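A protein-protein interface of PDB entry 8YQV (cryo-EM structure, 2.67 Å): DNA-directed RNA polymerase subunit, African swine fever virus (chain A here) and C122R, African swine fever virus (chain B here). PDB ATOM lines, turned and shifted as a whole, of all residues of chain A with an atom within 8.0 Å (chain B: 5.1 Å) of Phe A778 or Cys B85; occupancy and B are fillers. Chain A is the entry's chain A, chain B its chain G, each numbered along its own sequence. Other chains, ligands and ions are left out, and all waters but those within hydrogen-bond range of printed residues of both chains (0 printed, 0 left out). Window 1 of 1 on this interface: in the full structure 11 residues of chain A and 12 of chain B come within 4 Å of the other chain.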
ATOM      1  N   LEU A 684      21.047 -12.907 -23.197  1.00  0.00           N
ATOM      2  CA  LEU A 684      22.293 -13.219 -23.889  1.00  0.00           C
ATOM      3  C   LEU A 684      22.261 -12.758 -25.338  1.00  0.00           C
ATOM      4  O   LEU A 684      23.288 -12.327 -25.871  1.00  0.00           O
ATOM      5  CB  LEU A 684      22.563 -14.719 -23.826  1.00  0.00           C
ATOM      6  CG  LEU A 684      23.918 -15.186 -24.344  1.00  0.00           C
ATOM      7  CD1 LEU A 684      24.989 -14.923 -23.311  1.00  0.00           C
ATOM      8  CD2 LEU A 684      23.859 -16.649 -24.708  1.00  0.00           C
ATOM      9  N   LEU A 685      21.101 -12.847 -25.990  1.00  0.00           N
ATOM     10  CA  LEU A 685      20.990 -12.411 -27.378  1.00  0.00           C
ATOM     11  C   LEU A 685      21.282 -10.926 -27.520  1.00  0.00           C
ATOM     12  O   LEU A 685      21.939 -10.502 -28.477  1.00  0.00           O
ATOM     13  CB  LEU A 685      19.597 -12.728 -27.916  1.00  0.00           C
ATOM     14  CG  LEU A 685      19.505 -13.892 -28.895  1.00  0.00           C
ATOM     15  CD1 LEU A 685      20.024 -15.142 -28.246  1.00  0.00           C
ATOM     16  CD2 LEU A 685      18.070 -14.083 -29.347  1.00  0.00           C
ATOM     17  N   THR A 697      31.591 -14.236 -18.535  1.00  0.00           N
ATOM     18  CA  THR A 697      30.212 -14.284 -19.003  1.00  0.00           C
ATOM     19  C   THR A 697      29.713 -15.715 -19.120  1.00  0.00           C
ATOM     20  O   THR A 697      28.533 -15.980 -18.875  1.00  0.00           O
ATOM     21  CB  THR A 697      30.080 -13.568 -20.343  1.00  0.00           C
ATOM     22  OG1 THR A 697      30.581 -12.234 -20.217  1.00  0.00           O
ATOM     23  CG2 THR A 697      28.629 -13.503 -20.773  1.00  0.00           C
ATOM     24  N   HIS A 698      30.590 -16.651 -19.480  1.00  0.00           N
ATOM     25  CA  HIS A 698      30.175 -18.044 -19.595  1.00  0.00           C
ATOM     26  C   HIS A 698      29.769 -18.614 -18.242  1.00  0.00           C
ATOM     27  O   HIS A 698      28.717 -19.250 -18.117  1.00  0.00           O
ATOM     28  CB  HIS A 698      31.295 -18.875 -20.211  1.00  0.00           C
ATOM     29  CG  HIS A 698      30.964 -20.329 -20.337  1.00  0.00           C
ATOM     30  ND1 HIS A 698      30.205 -20.832 -21.369  1.00  0.00           N
ATOM     31  CD2 HIS A 698      31.278 -21.384 -19.550  1.00  0.00           C
ATOM     32  CE1 HIS A 698      30.072 -22.137 -21.218  1.00  0.00           C
ATOM     33  NE2 HIS A 698      30.712 -22.497 -20.121  1.00  0.00           N
ATOM     34  N   TYR A 701      26.572 -16.987 -16.973  1.00  0.00           N
ATOM     35  CA  TYR A 701      25.406 -17.448 -17.717  1.00  0.00           C
ATOM     36  C   TYR A 701      24.966 -18.829 -17.251  1.00  0.00           C
ATOM     37  O   TYR A 701      23.767 -19.095 -17.123  1.00  0.00           O
ATOM     38  CB  TYR A 701      25.717 -17.457 -19.210  1.00  0.00           C
ATOM     39  CG  TYR A 701      24.680 -18.125 -20.076  1.00  0.00           C
ATOM     40  CD1 TYR A 701      23.541 -17.450 -20.474  1.00  0.00           C
ATOM     41  CD2 TYR A 701      24.851 -19.430 -20.509  1.00  0.00           C
ATOM     42  CE1 TYR A 701      22.606 -18.057 -21.273  1.00  0.00           C
ATOM     43  CE2 TYR A 701      23.919 -20.040 -21.303  1.00  0.00           C
ATOM     44  CZ  TYR A 701      22.800 -19.352 -21.682  1.00  0.00           C
ATOM     45  OH  TYR A 701      21.868 -19.964 -22.477  1.00  0.00           O
ATOM     46  N   PRO A 764      29.389 -29.130 -23.579  1.00  0.00           N
ATOM     47  CA  PRO A 764      29.465 -29.603 -24.964  1.00  0.00           C
ATOM     48  C   PRO A 764      30.778 -30.292 -25.285  1.00  0.00           C
ATOM     49  O   PRO A 764      31.824 -29.651 -25.400  1.00  0.00           O
ATOM     50  CB  PRO A 764      29.288 -28.319 -25.783  1.00  0.00           C
ATOM     51  CG  PRO A 764      29.616 -27.223 -24.864  1.00  0.00           C
ATOM     52  CD  PRO A 764      29.198 -27.675 -23.507  1.00  0.00           C
ATOM     53  N   SER A 767      32.044 -31.960 -30.364  1.00  0.00           N
ATOM     54  CA  SER A 767      32.593 -31.065 -31.384  1.00  0.00           C
ATOM     55  C   SER A 767      32.140 -29.612 -31.208  1.00  0.00           C
ATOM     56  O   SER A 767      31.375 -29.071 -32.005  1.00  0.00           O
ATOM     57  CB  SER A 767      32.228 -31.534 -32.792  1.00  0.00           C
ATOM     58  OG  SER A 767      30.895 -31.186 -33.112  1.00  0.00           O
ATOM     59  N   PHE A 768      32.653 -28.987 -30.150  1.00  0.00           N
ATOM     60  CA  PHE A 768      32.736 -27.528 -30.090  1.00  0.00           C
ATOM     61  C   PHE A 768      31.349 -26.881 -30.154  1.00  0.00           C
ATOM     62  O   PHE A 768      30.942 -26.288 -31.150  1.00  0.00           O
ATOM     63  CB  PHE A 768      33.642 -26.990 -31.207  1.00  0.00           C
ATOM     64  CG  PHE A 768      33.658 -25.490 -31.305  1.00  0.00           C
ATOM     65  CD1 PHE A 768      34.051 -24.719 -30.229  1.00  0.00           C
ATOM     66  CD2 PHE A 768      33.279 -24.856 -32.472  1.00  0.00           C
ATOM     67  CE1 PHE A 768      34.061 -23.347 -30.313  1.00  0.00           C
ATOM     68  CE2 PHE A 768      33.289 -23.482 -32.562  1.00  0.00           C
ATOM     69  CZ  PHE A 768      33.682 -22.726 -31.482  1.00  0.00           C
ATOM     70  N   GLY A 769      30.609 -27.062 -29.073  1.00  0.00           N
ATOM     71  CA  GLY A 769      29.356 -26.366 -28.915  1.00  0.00           C
ATOM     72  C   GLY A 769      28.130 -27.214 -29.102  1.00  0.00           C
ATOM     73  O   GLY A 769      27.024 -26.665 -29.138  1.00  0.00           O
ATOM     74  N   ARG A 770      28.289 -28.524 -29.252  1.00  0.00           N
ATOM     75  CA  ARG A 770      27.184 -29.466 -29.259  1.00  0.00           C
ATOM     76  C   ARG A 770      27.359 -30.426 -28.099  1.00  0.00           C
ATOM     77  O   ARG A 770      28.472 -30.879 -27.821  1.00  0.00           O
ATOM     78  CB  ARG A 770      27.121 -30.259 -30.555  1.00  0.00           C
ATOM     79  CG  ARG A 770      27.396 -29.468 -31.797  1.00  0.00           C
ATOM     80  CD  ARG A 770      27.343 -30.374 -32.993  1.00  0.00           C
ATOM     81  NE  ARG A 770      25.977 -30.738 -33.331  1.00  0.00           N
ATOM     82  CZ  ARG A 770      25.650 -31.662 -34.219  1.00  0.00           C
ATOM     83  NH1 ARG A 770      26.571 -32.360 -34.856  1.00  0.00           N
ATOM     84  NH2 ARG A 770      24.369 -31.891 -34.475  1.00  0.00           N
ATOM     85  N   THR A 771      26.262 -30.721 -27.417  1.00  0.00           N
ATOM     86  CA  THR A 771      26.276 -31.731 -26.370  1.00  0.00           C
ATOM     87  C   THR A 771      25.955 -33.117 -26.903  1.00  0.00           C
ATOM     88  O   THR A 771      26.492 -34.105 -26.399  1.00  0.00           O
ATOM     89  CB  THR A 771      25.287 -31.351 -25.270  1.00  0.00           C
ATOM     90  OG1 THR A 771      23.997 -31.130 -25.848  1.00  0.00           O
ATOM     91  CG2 THR A 771      25.734 -30.085 -24.572  1.00  0.00           C
ATOM     92  N   TYR A 775      21.262 -31.990 -31.083  1.00  0.00           N
ATOM     93  CA  TYR A 775      21.084 -30.571 -30.862  1.00  0.00           C
ATOM     94  C   TYR A 775      22.095 -29.761 -31.658  1.00  0.00           C
ATOM     95  O   TYR A 775      23.266 -30.143 -31.741  1.00  0.00           O
ATOM     96  CB  TYR A 775      21.225 -30.243 -29.376  1.00  0.00           C
ATOM     97  CG  TYR A 775      20.205 -30.932 -28.516  1.00  0.00           C
ATOM     98  CD1 TYR A 775      18.873 -30.577 -28.579  1.00  0.00           C
ATOM     99  CD2 TYR A 775      20.572 -31.942 -27.646  1.00  0.00           C
ATOM    100  CE1 TYR A 775      17.939 -31.202 -27.803  1.00  0.00           C
ATOM    101  CE2 TYR A 775      19.642 -32.572 -26.863  1.00  0.00           C
ATOM    102  CZ  TYR A 775      18.327 -32.196 -26.945  1.00  0.00           C
ATOM    103  OH  TYR A 775      17.387 -32.822 -26.166  1.00  0.00           O
ATOM    104  N   PRO A 776      21.684 -28.641 -32.238  1.00  0.00           N
ATOM    105  CA  PRO A 776      22.595 -27.858 -33.073  1.00  0.00           C
ATOM    106  C   PRO A 776      23.694 -27.218 -32.247  1.00  0.00           C
ATOM    107  O   PRO A 776      23.649 -27.160 -31.020  1.00  0.00           O
ATOM    108  CB  PRO A 776      21.684 -26.806 -33.702  1.00  0.00           C
ATOM    109  CG  PRO A 776      20.576 -26.677 -32.767  1.00  0.00           C
ATOM    110  CD  PRO A 776      20.355 -28.023 -32.161  1.00  0.00           C
ATOM    111  N   ARG A 777      24.713 -26.752 -32.956  1.00  0.00           N
ATOM    112  CA  ARG A 777      25.837 -26.093 -32.313  1.00  0.00           C
ATOM    113  C   ARG A 777      25.378 -24.775 -31.704  1.00  0.00           C
ATOM    114  O   ARG A 777      24.608 -24.034 -32.320  1.00  0.00           O
ATOM    115  CB  ARG A 777      26.946 -25.862 -33.333  1.00  0.00           C
ATOM    116  CG  ARG A 777      28.289 -25.531 -32.744  1.00  0.00           C
ATOM    117  CD  ARG A 777      29.367 -25.576 -33.804  1.00  0.00           C
ATOM    118  NE  ARG A 777      29.825 -26.934 -34.060  1.00  0.00           N
ATOM    119  CZ  ARG A 777      29.943 -27.459 -35.270  1.00  0.00           C
ATOM    120  NH1 ARG A 777      29.672 -26.757 -36.355  1.00  0.00           N
ATOM    121  NH2 ARG A 777      30.341 -28.721 -35.392  1.00  0.00           N
ATOM    122  N   PHE A 778      25.854 -24.490 -30.490  1.00  0.00           N
ATOM    123  CA  PHE A 778      25.470 -23.298 -29.728  1.00  0.00           C
ATOM    124  C   PHE A 778      23.958 -23.231 -29.533  1.00  0.00           C
ATOM    125  O   PHE A 778      23.340 -22.173 -29.647  1.00  0.00           O
ATOM    126  CB  PHE A 778      25.982 -22.016 -30.390  1.00  0.00           C
ATOM    127  CG  PHE A 778      27.397 -22.101 -30.851  1.00  0.00           C
ATOM    128  CD1 PHE A 778      28.404 -22.412 -29.966  1.00  0.00           C
ATOM    129  CD2 PHE A 778      27.718 -21.861 -32.169  1.00  0.00           C
ATOM    130  CE1 PHE A 778      29.699 -22.498 -30.390  1.00  0.00           C
ATOM    131  CE2 PHE A 778      29.011 -21.945 -32.593  1.00  0.00           C
ATOM    132  CZ  PHE A 778      30.002 -22.262 -31.705  1.00  0.00           C
ATOM    133  N   ALA A 779      23.359 -24.380 -29.249  1.00  0.00           N
ATOM    134  CA  ALA A 779      21.939 -24.413 -28.945  1.00  0.00           C
ATOM    135  C   ALA A 779      21.680 -23.722 -27.615  1.00  0.00           C
ATOM    136  O   ALA A 779      22.446 -23.859 -26.661  1.00  0.00           O
ATOM    137  CB  ALA A 779      21.431 -25.851 -28.901  1.00  0.00           C
ATOM    138  N   LEU A 780      20.593 -22.962 -27.560  1.00  0.00           N
ATOM    139  CA  LEU A 780      20.275 -22.187 -26.375  1.00  0.00           C
ATOM    140  C   LEU A 780      19.165 -22.791 -25.534  1.00  0.00           C
ATOM    141  O   LEU A 780      18.978 -22.363 -24.392  1.00  0.00           O
ATOM    142  CB  LEU A 780      19.889 -20.757 -26.770  1.00  0.00           C
ATOM    143  CG  LEU A 780      21.028 -19.895 -27.304  1.00  0.00           C
ATOM    144  CD1 LEU A 780      20.483 -18.562 -27.724  1.00  0.00           C
ATOM    145  CD2 LEU A 780      22.114 -19.729 -26.260  1.00  0.00           C
ATOM    146  N   GLU A 781      18.437 -23.770 -26.055  1.00  0.00           N
ATOM    147  CA  GLU A 781      17.378 -24.403 -25.290  1.00  0.00           C
ATOM    148  C   GLU A 781      17.960 -25.141 -24.092  1.00  0.00           C
ATOM    149  O   GLU A 781      19.108 -25.585 -24.106  1.00  0.00           O
ATOM    150  CB  GLU A 781      16.588 -25.360 -26.178  1.00  0.00           C
ATOM    151  CG  GLU A 781      17.375 -26.574 -26.629  1.00  0.00           C
ATOM    152  CD  GLU A 781      17.475 -26.679 -28.134  1.00  0.00           C
ATOM    153  OE1 GLU A 781      17.700 -25.641 -28.789  1.00  0.00           O
ATOM    154  OE2 GLU A 781      17.326 -27.799 -28.663  1.00  0.00           O
ATOM    155  N   ALA A 784      19.027 -28.975 -24.413  1.00  0.00           N
ATOM    156  CA  ALA A 784      20.304 -29.317 -25.017  1.00  0.00           C
ATOM    157  C   ALA A 784      21.390 -29.581 -23.993  1.00  0.00           C
ATOM    158  O   ALA A 784      22.430 -30.131 -24.355  1.00  0.00           O
ATOM    159  CB  ALA A 784      20.750 -28.206 -25.961  1.00  0.00           C
ATOM    160  N   TYR A 785      21.176 -29.217 -22.731  1.00  0.00           N
ATOM    161  CA  TYR A 785      22.216 -29.318 -21.719  1.00  0.00           C
ATOM    162  C   TYR A 785      21.803 -30.159 -20.524  1.00  0.00           C
ATOM    163  O   TYR A 785      22.458 -30.085 -19.483  1.00  0.00           O
ATOM    164  CB  TYR A 785      22.637 -27.929 -21.247  1.00  0.00           C
ATOM    165  CG  TYR A 785      23.065 -27.049 -22.381  1.00  0.00           C
ATOM    166  CD1 TYR A 785      24.385 -26.993 -22.777  1.00  0.00           C
ATOM    167  CD2 TYR A 785      22.143 -26.288 -23.070  1.00  0.00           C
ATOM    168  CE1 TYR A 785      24.772 -26.203 -23.819  1.00  0.00           C
ATOM    169  CE2 TYR A 785      22.519 -25.501 -24.108  1.00  0.00           C
ATOM    170  CZ  TYR A 785      23.833 -25.458 -24.481  1.00  0.00           C
ATOM    171  OH  TYR A 785      24.210 -24.655 -25.526  1.00  0.00           O
ATOM    172  N   PHE B  56      35.833 -20.433 -39.136  1.00  0.00           N
ATOM    173  CA  PHE B  56      34.566 -20.942 -38.638  1.00  0.00           C
ATOM    174  C   PHE B  56      33.435 -19.953 -38.864  1.00  0.00           C
ATOM    175  O   PHE B  56      32.330 -20.353 -39.244  1.00  0.00           O
ATOM    176  CB  PHE B  56      34.688 -21.277 -37.156  1.00  0.00           C
ATOM    177  CG  PHE B  56      33.407 -21.728 -36.538  1.00  0.00           C
ATOM    178  CD1 PHE B  56      32.943 -23.012 -36.741  1.00  0.00           C
ATOM    179  CD2 PHE B  56      32.657 -20.865 -35.759  1.00  0.00           C
ATOM    180  CE1 PHE B  56      31.762 -23.426 -36.179  1.00  0.00           C
ATOM    181  CE2 PHE B  56      31.476 -21.276 -35.197  1.00  0.00           C
ATOM    182  CZ  PHE B  56      31.028 -22.557 -35.406  1.00  0.00           C
ATOM    183  N   ASN B  66      24.541 -25.637 -37.338  1.00  0.00           N
ATOM    184  CA  ASN B  66      24.559 -24.384 -36.602  1.00  0.00           C
ATOM    185  C   ASN B  66      23.145 -23.951 -36.241  1.00  0.00           C
ATOM    186  O   ASN B  66      22.171 -24.316 -36.904  1.00  0.00           O
ATOM    187  CB  ASN B  66      25.245 -23.286 -37.411  1.00  0.00           C
ATOM    188  CG  ASN B  66      26.736 -23.278 -37.225  1.00  0.00           C
ATOM    189  OD1 ASN B  66      27.238 -23.600 -36.153  1.00  0.00           O
ATOM    190  ND2 ASN B  66      27.456 -22.886 -38.261  1.00  0.00           N
ATOM    191  N   CYS B  67      23.045 -23.160 -35.177  1.00  0.00           N
ATOM    192  CA  CYS B  67      21.754 -22.720 -34.670  1.00  0.00           C
ATOM    193  C   CYS B  67      21.253 -21.541 -35.493  1.00  0.00           C
ATOM    194  O   CYS B  67      21.950 -20.532 -35.628  1.00  0.00           O
ATOM    195  CB  CYS B  67      21.869 -22.345 -33.198  1.00  0.00           C
ATOM    196  SG  CYS B  67      20.317 -21.863 -32.431  1.00  0.00           S
ATOM    197  N   GLN B  83      23.120 -18.004 -35.844  1.00  0.00           N
ATOM    198  CA  GLN B  83      23.690 -17.454 -34.626  1.00  0.00           C
ATOM    199  C   GLN B  83      24.833 -18.322 -34.125  1.00  0.00           C
ATOM    200  O   GLN B  83      24.709 -19.546 -34.047  1.00  0.00           O
ATOM    201  CB  GLN B  83      22.618 -17.319 -33.547  1.00  0.00           C
ATOM    202  CG  GLN B  83      23.133 -17.458 -32.130  1.00  0.00           C
ATOM    203  CD  GLN B  83      22.530 -18.651 -31.424  1.00  0.00           C
ATOM    204  OE1 GLN B  83      21.334 -18.910 -31.538  1.00  0.00           O
ATOM    205  NE2 GLN B  83      23.357 -19.394 -30.699  1.00  0.00           N
ATOM    206  N   ILE B  84      25.955 -17.683 -33.798  1.00  0.00           N
ATOM    207  CA  ILE B  84      27.091 -18.370 -33.199  1.00  0.00           C
ATOM    208  C   ILE B  84      27.502 -17.631 -31.937  1.00  0.00           C
ATOM    209  O   ILE B  84      27.530 -16.399 -31.895  1.00  0.00           O
ATOM    210  CB  ILE B  84      28.289 -18.503 -34.166  1.00  0.00           C
ATOM    211  CG1 ILE B  84      28.615 -17.166 -34.821  1.00  0.00           C
ATOM    212  CG2 ILE B  84      28.002 -19.548 -35.226  1.00  0.00           C
ATOM    213  CD1 ILE B  84      29.516 -17.287 -36.024  1.00  0.00           C
ATOM    214  N   CYS B  85      27.822 -18.397 -30.898  1.00  0.00           N
ATOM    215  CA  CYS B  85      28.152 -17.867 -29.575  1.00  0.00           C
ATOM    216  C   CYS B  85      29.560 -18.331 -29.223  1.00  0.00           C
ATOM    217  O   CYS B  85      29.747 -19.423 -28.682  1.00  0.00           O
ATOM    218  CB  CYS B  85      27.134 -18.328 -28.549  1.00  0.00           C
ATOM    219  SG  CYS B  85      27.399 -17.691 -26.901  1.00  0.00           S
ATOM    220  N   ILE B  86      30.545 -17.496 -29.504  1.00  0.00           N
ATOM    221  CA  ILE B  86      31.940 -17.907 -29.401  1.00  0.00           C
ATOM    222  C   ILE B  86      32.578 -17.305 -28.158  1.00  0.00           C
ATOM    223  O   ILE B  86      32.206 -16.223 -27.695  1.00  0.00           O
ATOM    224  CB  ILE B  86      32.744 -17.518 -30.657  1.00  0.00           C
ATOM    225  CG1 ILE B  86      32.589 -16.024 -30.937  1.00  0.00           C
ATOM    226  CG2 ILE B  86      32.304 -18.348 -31.855  1.00  0.00           C
ATOM    227  CD1 ILE B  86      32.959 -15.637 -32.332  1.00  0.00           C
ATOM    228  N   GLY B  87      33.560 -18.023 -27.620  1.00  0.00           N
ATOM    229  CA  GLY B  87      34.382 -17.514 -26.545  1.00  0.00           C
ATOM    230  C   GLY B  87      33.746 -17.645 -25.180  1.00  0.00           C
ATOM    231  O   GLY B  87      32.586 -18.025 -25.019  1.00  0.00           O
ATOM    232  N   LYS B  90      31.017 -15.198 -24.490  1.00  0.00           N
ATOM    233  CA  LYS B  90      29.781 -15.556 -25.178  1.00  0.00           C
ATOM    234  C   LYS B  90      29.345 -14.450 -26.136  1.00  0.00           C
ATOM    235  O   LYS B  90      28.295 -13.829 -25.979  1.00  0.00           O
ATOM    236  CB  LYS B  90      28.675 -15.891 -24.178  1.00  0.00           C
ATOM    237  CG  LYS B  90      28.985 -17.083 -23.298  1.00  0.00           C
ATOM    238  CD  LYS B  90      27.764 -17.513 -22.519  1.00  0.00           C
ATOM    239  CE  LYS B  90      26.826 -18.323 -23.387  1.00  0.00           C
ATOM    240  NZ  LYS B  90      27.390 -19.665 -23.693  1.00  0.00           N
ATOM    241  N   ILE B  91      30.182 -14.205 -27.133  1.00  0.00           N
ATOM    242  CA  ILE B  91      29.880 -13.210 -28.152  1.00  0.00           C
ATOM    243  C   ILE B  91      28.921 -13.816 -29.166  1.00  0.00           C
ATOM    244  O   ILE B  91      29.169 -14.905 -29.696  1.00  0.00           O
ATOM    245  CB  ILE B  91      31.167 -12.715 -28.827  1.00  0.00           C
ATOM    246  CG1 ILE B  91      32.155 -12.223 -27.776  1.00  0.00           C
ATOM    247  CG2 ILE B  91      30.858 -11.613 -29.815  1.00  0.00           C
ATOM    248  CD1 ILE B  91      31.630 -11.088 -26.929  1.00  0.00           C
ATOM    249  N   ILE B  92      27.828 -13.109 -29.435  1.00  0.00           N
ATOM    250  CA  ILE B  92      26.796 -13.563 -30.359  1.00  0.00           C
ATOM    251  C   ILE B  92      27.018 -12.882 -31.703  1.00  0.00           C
ATOM    252  O   ILE B  92      27.130 -11.656 -31.774  1.00  0.00           O
ATOM    253  CB  ILE B  92      25.393 -13.256 -29.818  1.00  0.00           C
ATOM    254  CG1 ILE B  92      25.104 -14.071 -28.559  1.00  0.00           C
ATOM    255  CG2 ILE B  92      24.341 -13.521 -30.874  1.00  0.00           C
ATOM    256  CD1 ILE B  92      24.871 -15.530 -28.811  1.00  0.00           C
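The backbone carbonyl oxygen (O) of Arg A777 lies close to the backbone NH (N) of Cys B67 (3.4 Å). O of Phe A778 sits at hydrogen-bond distance from NE2 of Gln B83 (3.0 Å).
Of chain B, only Phe B56 (3.5 Å), Cys B67 (3.8 Å), Gln B83 (3.0 Å), Ile B84 (3.7 Å) and Cys B85 (3.5 Å) come within 4 Å of Phe A778. Printed residues of chain A within 4 Å of Cys B85: Phe A778. Of the printed residues of chain A, Lys B90 touches Leu A684, His A698 and Tyr A701. Of the printed residues of chain B, His A698 touches Lys B90 (3.8 Å). Of the printed residues of chain B, Phe A768 touches Phe B56. Printed residues of chain B within 4 Å of Leu A684: Lys B90 (3.7 Å) and Ile B92 (3.7 Å). Of the printed residues of chain A, Asn B66 touches Arg A777 (3.6 Å). Ser A767 touches none of the printed residues of chain B.
The backbone carbonyl oxygen of Ser A767 is in hydrogen-bond range of the guanidinium group of Arg A777, at 3.3 Å. The backbone carbonyl oxygen (O) of Phe A768 lies close to the guanidinium group (NE) of Arg A777 (3.2 Å). The backbone NH of Phe A778 is in hydrogen-bond range of the backbone carbonyl oxygen of Gly A769 (2.8 Å). The backbone carbonyl oxygen of Cys B67 sits at hydrogen-bond distance from the backbone NH of Gln B83 (2.8 Å). The side-chain sulfur of Cys B85 lies close to the side-chain amino group of Lys B90 (3.8 Å).
Hydrophobic or aromatic side chains of chain A that line the printed part of chain B: Leu A684, His A698, Tyr A701, Phe A768, Phe A778 and Leu A780. Along chain A the printed residues that touch a printed residue of chain B span positions 684 to 780. Hydrophobic or aromatic side chains of chain B that line the printed part of chain A: Phe B56, Ile B84 and Ile B92. Along chain B the printed residues that touch a printed residue of chain A span positions 56 to 92. Among the printed residues, no Asp or Glu carboxylate lies within 4 Å of a Lys or Arg side-chain nitrogen of the other chain.
Among the printed residues, pairs that only touch across the chains: Phe A778 with Phe B56 (3.5 Å), Phe A778 with Cys B85 (3.5 Å), Arg A777 with Asn B66 (3.6 Å), Leu A684 with Lys B90 (3.7 Å), Tyr A701 with Lys B90 (3.7 Å), Leu A684 with Ile B92 (3.7 Å), Phe A778 with Ile B84 (3.7 Å), Phe A768 with Phe B56 (3.7 Å), Arg A777 with Phe B56 (3.8 Å), His A698 with Lys B90 (3.8 Å), Phe A778 with Cys B67 (3.8 Å) and Leu A780 with Gln B83 (3.9 Å).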
